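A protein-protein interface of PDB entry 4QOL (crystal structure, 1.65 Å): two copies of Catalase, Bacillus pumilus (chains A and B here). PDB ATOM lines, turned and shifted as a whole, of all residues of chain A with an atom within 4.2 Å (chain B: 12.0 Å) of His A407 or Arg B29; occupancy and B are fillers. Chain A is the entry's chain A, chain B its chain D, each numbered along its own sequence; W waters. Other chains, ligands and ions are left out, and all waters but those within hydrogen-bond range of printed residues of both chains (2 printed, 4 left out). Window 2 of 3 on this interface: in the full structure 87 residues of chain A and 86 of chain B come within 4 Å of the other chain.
No position is printed for both chains.
Of the 8 pairs that touch across the chains among the printed residues, none has its exchanged pair printed and touching as well.
A ring nitrogen (NE2) of His A407 sits close to the guanidinium group of Arg B29, 3.4 Å away.
Water W2 lies within hydrogen-bond range of O of Gly B30 (2.7 Å), O of Glu A329 (2.9 Å) and OG of Ser B32 (3.0 Å).
Water W1 lies within hydrogen-bond range of the guanidinium group of Arg B29, the side-chain carboxylate of Glu A329 and the side-chain carboxylate of Asp A277.
The backbone carbonyl oxygen (O) of Gly B27 lies within hydrogen-bond range of the side-chain hydroxyl (OG1) of Thr B25 (2.6 Å).
The backbone NH of Ala B26 lies within hydrogen-bond range of the backbone carbonyl oxygen of Pro B31 (3.0 Å).
Among the printed residues, merely in contact across the chains: Tyr A271 with Arg B29 (3.2 Å), Glu A329 with Arg B29 (3.5 Å), Glu A329 with Gly B30 (3.7 Å), Glu A329 with Pro B31 (3.9 Å), Leu A406 with Pro B31 (3.8 Å), Gly A408 with Ala B26 (3.9 Å) and Gly A408 with Gly B27 (3.7 Å).
Of the 8 printed residues of chain A, 5 touch a printed residue of chain B.
Of the 12 printed residues of chain B, 5 touch a printed residue of chain A.
Along chain B the printed residues that touch a printed residue of chain A span positions 26 to 31.
Among the printed residues, 8 pairs touch across the chains.
Among the printed residues, no Asp or Glu carboxylate lies within 4 Å of a Lys or Arg side-chain nitrogen of the other chain.
Of chain B, only Arg B29 (3.5 Å), Gly B30 (3.7 Å) and Pro B31 (3.9 Å) come within 4 Å of Glu A329.
His A407 touches just one residue of chain B: Arg B29 (3.0 Å).
Gly A408 touches just these residues of chain B: Ala B26 (3.9 Å) and Gly B27 (3.7 Å).
Asn B22 touches none of the printed residues of chain A.
Ser B23 touches none of the printed residues of chain A.
Printed residues of chain A within 4 Å of Ala B26: Gly A408 (3.9 Å).
Of the printed residues of chain A, Gly B27 touches Gly A408.
Arg B29 touches three residues of chain A.
Of the printed residues of chain A, Gly B30 touches Glu A329.
The nearest residue of chain A that does not touch Arg B29 is Asp A277 (4.02 Å).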
ATOM      1  N   TYR A 271     -12.315  -4.998   1.596  1.00  0.00           N
ATOM      2  CA  TYR A 271     -12.743  -4.884   0.186  1.00  0.00           C
ATOM      3  C   TYR A 271     -12.111  -5.969  -0.616  1.00  0.00           C
ATOM      4  O   TYR A 271     -12.756  -6.679  -1.417  1.00  0.00           O
ATOM      5  CB  TYR A 271     -12.323  -3.535  -0.451  1.00  0.00           C
ATOM      6  CG  TYR A 271     -12.557  -3.520  -1.987  1.00  0.00           C
ATOM      7  CD1 TYR A 271     -13.790  -3.150  -2.528  1.00  0.00           C
ATOM      8  CD2 TYR A 271     -11.565  -3.922  -2.880  1.00  0.00           C
ATOM      9  CE1 TYR A 271     -14.016  -3.156  -3.898  1.00  0.00           C
ATOM     10  CE2 TYR A 271     -11.786  -3.974  -4.252  1.00  0.00           C
ATOM     11  CZ  TYR A 271     -13.006  -3.562  -4.770  1.00  0.00           C
ATOM     12  OH  TYR A 271     -13.260  -3.568  -6.149  1.00  0.00           O
ATOM     13  N   ASP A 277     -18.180  -6.050  -4.310  1.00  0.00           N
ATOM     14  CA  ASP A 277     -17.814  -4.700  -3.808  1.00  0.00           C
ATOM     15  C   ASP A 277     -18.691  -4.358  -2.591  1.00  0.00           C
ATOM     16  O   ASP A 277     -19.913  -4.334  -2.688  1.00  0.00           O
ATOM     17  CB  ASP A 277     -18.001  -3.664  -4.922  1.00  0.00           C
ATOM     18  CG  ASP A 277     -17.594  -2.276  -4.538  1.00  0.00           C
ATOM     19  OD1 ASP A 277     -17.606  -1.903  -3.339  1.00  0.00           O
ATOM     20  OD2 ASP A 277     -17.256  -1.553  -5.455  1.00  0.00           O
ATOM     21  N   GLU A 329     -18.058   5.684  -1.083  1.00  0.00           N
ATOM     22  CA  GLU A 329     -17.924   5.777  -2.543  1.00  0.00           C
ATOM     23  C   GLU A 329     -19.069   5.191  -3.396  1.00  0.00           C
ATOM     24  O   GLU A 329     -19.079   5.358  -4.611  1.00  0.00           O
ATOM     25  CB  GLU A 329     -16.555   5.165  -2.879  1.00  0.00           C
ATOM     26  CG  GLU A 329     -16.352   3.820  -2.170  1.00  0.00           C
ATOM     27  CD  GLU A 329     -15.655   3.784  -0.713  1.00  0.00           C
ATOM     28  OE1 GLU A 329     -15.766   4.600   0.240  1.00  0.00           O
ATOM     29  OE2 GLU A 329     -14.966   2.759  -0.433  1.00  0.00           O
ATOM     30  N   VAL A 405      -8.922   7.771   0.763  1.00  0.00           N
ATOM     31  CA  VAL A 405      -7.978   7.374  -0.228  1.00  0.00           C
ATOM     32  C   VAL A 405      -8.704   7.044  -1.521  1.00  0.00           C
ATOM     33  O   VAL A 405      -9.765   6.387  -1.522  1.00  0.00           O
ATOM     34  CB  VAL A 405      -7.156   6.166   0.255  1.00  0.00           C
ATOM     35  CG1 VAL A 405      -6.331   5.600  -0.893  1.00  0.00           C
ATOM     36  CG2 VAL A 405      -6.215   6.626   1.385  1.00  0.00           C
ATOM     37  N   LEU A 406      -8.141   7.503  -2.632  1.00  0.00           N
ATOM     38  CA  LEU A 406      -8.675   7.211  -3.949  1.00  0.00           C
ATOM     39  C   LEU A 406      -7.833   6.104  -4.565  1.00  0.00           C
ATOM     40  O   LEU A 406      -6.593   6.149  -4.528  1.00  0.00           O
ATOM     41  CB  LEU A 406      -8.581   8.447  -4.842  1.00  0.00           C
ATOM     42  CG  LEU A 406      -9.279   9.717  -4.297  1.00  0.00           C
ATOM     43  CD1 LEU A 406      -8.869  10.937  -5.101  1.00  0.00           C
ATOM     44  CD2 LEU A 406     -10.779   9.506  -4.294  1.00  0.00           C
ATOM     45  N   HIS A 407      -8.504   5.124  -5.121  1.00  0.00           N
ATOM     46  CA  HIS A 407      -7.811   4.015  -5.714  1.00  0.00           C
ATOM     47  C   HIS A 407      -7.639   4.244  -7.217  1.00  0.00           C
ATOM     48  O   HIS A 407      -6.719   3.698  -7.830  1.00  0.00           O
ATOM     49  CB  HIS A 407      -8.520   2.710  -5.333  1.00  0.00           C
ATOM     50  CG  HIS A 407      -8.567   2.497  -3.851  1.00  0.00           C
ATOM     51  ND1 HIS A 407      -7.438   2.210  -3.106  1.00  0.00           N
ATOM     52  CD2 HIS A 407      -9.578   2.627  -2.961  1.00  0.00           C
ATOM     53  CE1 HIS A 407      -7.760   2.147  -1.827  1.00  0.00           C
ATOM     54  NE2 HIS A 407      -9.057   2.370  -1.715  1.00  0.00           N
ATOM     55  N   GLY A 408      -8.472   5.083  -7.802  1.00  0.00           N
ATOM     56  CA  GLY A 408      -8.374   5.356  -9.224  1.00  0.00           C
ATOM     57  C   GLY A 408      -7.412   6.447  -9.599  1.00  0.00           C
ATOM     58  O   GLY A 408      -7.177   7.380  -8.845  1.00  0.00           O
ATOM     59  N   ASP A 409      -6.883   6.342 -10.797  1.00  0.00           N
ATOM     60  CA  ASP A 409      -5.896   7.293 -11.286  1.00  0.00           C
ATOM     61  C   ASP A 409      -6.418   8.201 -12.416  1.00  0.00           C
ATOM     62  O   ASP A 409      -5.683   9.109 -12.875  1.00  0.00           O
ATOM     63  CB  ASP A 409      -4.649   6.531 -11.741  1.00  0.00           C
ATOM     64  CG  ASP A 409      -4.712   6.122 -13.185  1.00  0.00           C
ATOM     65  OD1 ASP A 409      -5.512   5.193 -13.493  1.00  0.00           O
ATOM     66  OD2 ASP A 409      -3.933   6.726 -14.011  1.00  0.00           O
ATOM     67  N   ASN B  22     -23.099   4.952 -16.518  1.00  0.00           N
ATOM     68  CA  ASN B  22     -22.156   5.210 -15.430  1.00  0.00           C
ATOM     69  C   ASN B  22     -21.938   6.693 -15.209  1.00  0.00           C
ATOM     70  O   ASN B  22     -21.591   7.425 -16.144  1.00  0.00           O
ATOM     71  CB  ASN B  22     -20.776   4.545 -15.698  1.00  0.00           C
ATOM     72  CG  ASN B  22     -20.891   3.074 -16.044  1.00  0.00           C
ATOM     73  OD1 ASN B  22     -21.258   2.259 -15.195  1.00  0.00           O
ATOM     74  ND2 ASN B  22     -20.671   2.740 -17.333  1.00  0.00           N
ATOM     75  N   SER B  23     -21.984   7.076 -13.938  1.00  0.00           N
ATOM     76  CA  SER B  23     -21.512   8.379 -13.471  1.00  0.00           C
ATOM     77  C   SER B  23     -19.981   8.487 -13.675  1.00  0.00           C
ATOM     78  O   SER B  23     -19.303   7.474 -13.780  1.00  0.00           O
ATOM     79  CB  SER B  23     -21.817   8.507 -11.995  1.00  0.00           C
ATOM     80  OG  SER B  23     -23.161   8.538 -11.706  1.00  0.00           O
ATOM     81  N   ARG B  24     -19.470   9.709 -13.703  1.00  0.00           N
ATOM     82  CA  ARG B  24     -18.058   9.955 -13.792  1.00  0.00           C
ATOM     83  C   ARG B  24     -17.407  10.000 -12.387  1.00  0.00           C
ATOM     84  O   ARG B  24     -17.830  10.774 -11.509  1.00  0.00           O
ATOM     85  CB  ARG B  24     -17.891  11.269 -14.519  1.00  0.00           C
ATOM     86  CG  ARG B  24     -16.519  11.525 -15.007  1.00  0.00           C
ATOM     87  CD  ARG B  24     -16.553  12.809 -15.781  1.00  0.00           C
ATOM     88  NE  ARG B  24     -15.439  12.826 -16.698  1.00  0.00           N
ATOM     89  CZ  ARG B  24     -14.929  13.924 -17.197  1.00  0.00           C
ATOM     90  NH1 ARG B  24     -15.420  15.128 -16.825  1.00  0.00           N
ATOM     91  NH2 ARG B  24     -13.921  13.828 -18.054  1.00  0.00           N
ATOM     92  N   THR B  25     -16.361   9.177 -12.188  1.00  0.00           N
ATOM     93  CA  THR B  25     -15.899   8.842 -10.862  1.00  0.00           C
ATOM     94  C   THR B  25     -14.375   8.732 -10.853  1.00  0.00           C
ATOM     95  O   THR B  25     -13.731   8.689 -11.899  1.00  0.00           O
ATOM     96  CB  THR B  25     -16.484   7.485 -10.375  1.00  0.00           C
ATOM     97  OG1 THR B  25     -16.132   6.408 -11.283  1.00  0.00           O
ATOM     98  CG2 THR B  25     -17.987   7.542 -10.254  1.00  0.00           C
ATOM     99  N   ALA B  26     -13.826   8.761  -9.657  1.00  0.00           N
ATOM    100  CA  ALA B  26     -12.374   8.599  -9.477  1.00  0.00           C
ATOM    101  C   ALA B  26     -12.034   7.119  -9.556  1.00  0.00           C
ATOM    102  O   ALA B  26     -12.120   6.413  -8.557  1.00  0.00           O
ATOM    103  CB  ALA B  26     -11.950   9.212  -8.160  1.00  0.00           C
ATOM    104  N   GLY B  27     -11.700   6.672 -10.766  1.00  0.00           N
ATOM    105  CA  GLY B  27     -11.609   5.237 -11.072  1.00  0.00           C
ATOM    106  C   GLY B  27     -12.980   4.532 -11.066  1.00  0.00           C
ATOM    107  O   GLY B  27     -14.009   5.110 -10.700  1.00  0.00           O
ATOM    108  N   HIS B  28     -12.975   3.238 -11.370  1.00  0.00           N
ATOM    109  CA  HIS B  28     -14.210   2.486 -11.466  1.00  0.00           C
ATOM    110  C   HIS B  28     -14.969   2.303 -10.145  1.00  0.00           C
ATOM    111  O   HIS B  28     -16.174   2.011 -10.196  1.00  0.00           O
ATOM    112  CB  HIS B  28     -14.012   1.116 -12.119  1.00  0.00           C
ATOM    113  CG  HIS B  28     -13.015   0.262 -11.419  1.00  0.00           C
ATOM    114  ND1 HIS B  28     -11.765  -0.009 -11.938  1.00  0.00           N
ATOM    115  CD2 HIS B  28     -13.047  -0.303 -10.191  1.00  0.00           C
ATOM    116  CE1 HIS B  28     -11.080  -0.723 -11.059  1.00  0.00           C
ATOM    117  NE2 HIS B  28     -11.838  -0.923  -9.994  1.00  0.00           N
ATOM    118  N   ARG B  29     -14.332   2.509  -8.995  1.00  0.00           N
ATOM    119  CA  ARG B  29     -15.046   2.375  -7.750  1.00  0.00           C
ATOM    120  C   ARG B  29     -14.987   3.542  -6.815  1.00  0.00           C
ATOM    121  O   ARG B  29     -15.194   3.396  -5.584  1.00  0.00           O
ATOM    122  CB  ARG B  29     -14.668   1.087  -7.035  1.00  0.00           C
ATOM    123  CG  ARG B  29     -13.216   0.975  -6.597  1.00  0.00           C
ATOM    124  CD  ARG B  29     -13.040  -0.357  -5.864  1.00  0.00           C
ATOM    125  NE  ARG B  29     -11.769  -0.522  -5.144  1.00  0.00           N
ATOM    126  CZ  ARG B  29     -11.559  -0.059  -3.906  1.00  0.00           C
ATOM    127  NH1 ARG B  29     -12.502   0.662  -3.291  1.00  0.00           N
ATOM    128  NH2 ARG B  29     -10.401  -0.290  -3.296  1.00  0.00           N
ATOM    129  N   GLY B  30     -14.709   4.726  -7.347  1.00  0.00           N
ATOM    130  CA  GLY B  30     -14.374   5.861  -6.441  1.00  0.00           C
ATOM    131  C   GLY B  30     -15.577   6.749  -6.389  1.00  0.00           C
ATOM    132  O   GLY B  30     -16.607   6.511  -7.095  1.00  0.00           O
ATOM    133  N   PRO B  31     -15.499   7.801  -5.564  1.00  0.00           N
ATOM    134  CA  PRO B  31     -16.560   8.810  -5.527  1.00  0.00           C
ATOM    135  C   PRO B  31     -16.714   9.636  -6.806  1.00  0.00           C
ATOM    136  O   PRO B  31     -15.888   9.604  -7.721  1.00  0.00           O
ATOM    137  CB  PRO B  31     -16.112   9.734  -4.363  1.00  0.00           C
ATOM    138  CG  PRO B  31     -14.654   9.637  -4.407  1.00  0.00           C
ATOM    139  CD  PRO B  31     -14.339   8.206  -4.774  1.00  0.00           C
ATOM    140  N   SER B  32     -17.849  10.346  -6.891  1.00  0.00           N
ATOM    141  CA  SER B  32     -18.323  10.950  -8.123  1.00  0.00           C
ATOM    142  C   SER B  32     -17.867  12.365  -8.284  1.00  0.00           C
ATOM    143  O   SER B  32     -17.757  13.105  -7.307  1.00  0.00           O
ATOM    144  CB  SER B  32     -19.871  10.899  -8.166  1.00  0.00           C
ATOM    145  OG  SER B  32     -20.345   9.578  -8.321  1.00  0.00           O
ATOM    146  N   PHE B  33     -17.644  12.755  -9.538  1.00  0.00           N
ATOM    147  CA  PHE B  33     -17.192  14.080  -9.810  1.00  0.00           C
ATOM    148  C   PHE B  33     -18.335  15.048 -10.135  1.00  0.00           C
ATOM    149  O   PHE B  33     -19.400  14.655 -10.687  1.00  0.00           O
ATOM    150  CB  PHE B  33     -16.194  14.113 -10.958  1.00  0.00           C
ATOM    151  CG  PHE B  33     -14.850  13.608 -10.576  1.00  0.00           C
ATOM    152  CD1 PHE B  33     -14.051  14.329  -9.735  1.00  0.00           C
ATOM    153  CD2 PHE B  33     -14.401  12.371 -11.025  1.00  0.00           C
ATOM    154  CE1 PHE B  33     -12.806  13.872  -9.316  1.00  0.00           C
ATOM    155  CE2 PHE B  33     -13.145  11.909 -10.661  1.00  0.00           C
ATOM    156  CZ  PHE B  33     -12.333  12.647  -9.789  1.00  0.00           C
HETATM  157  O   HOH W   1     -14.940   0.015  -2.198  1.00  0.00           O
HETATM  158  O   HOH W   2     -19.170   7.387  -6.716  1.00  0.00           O
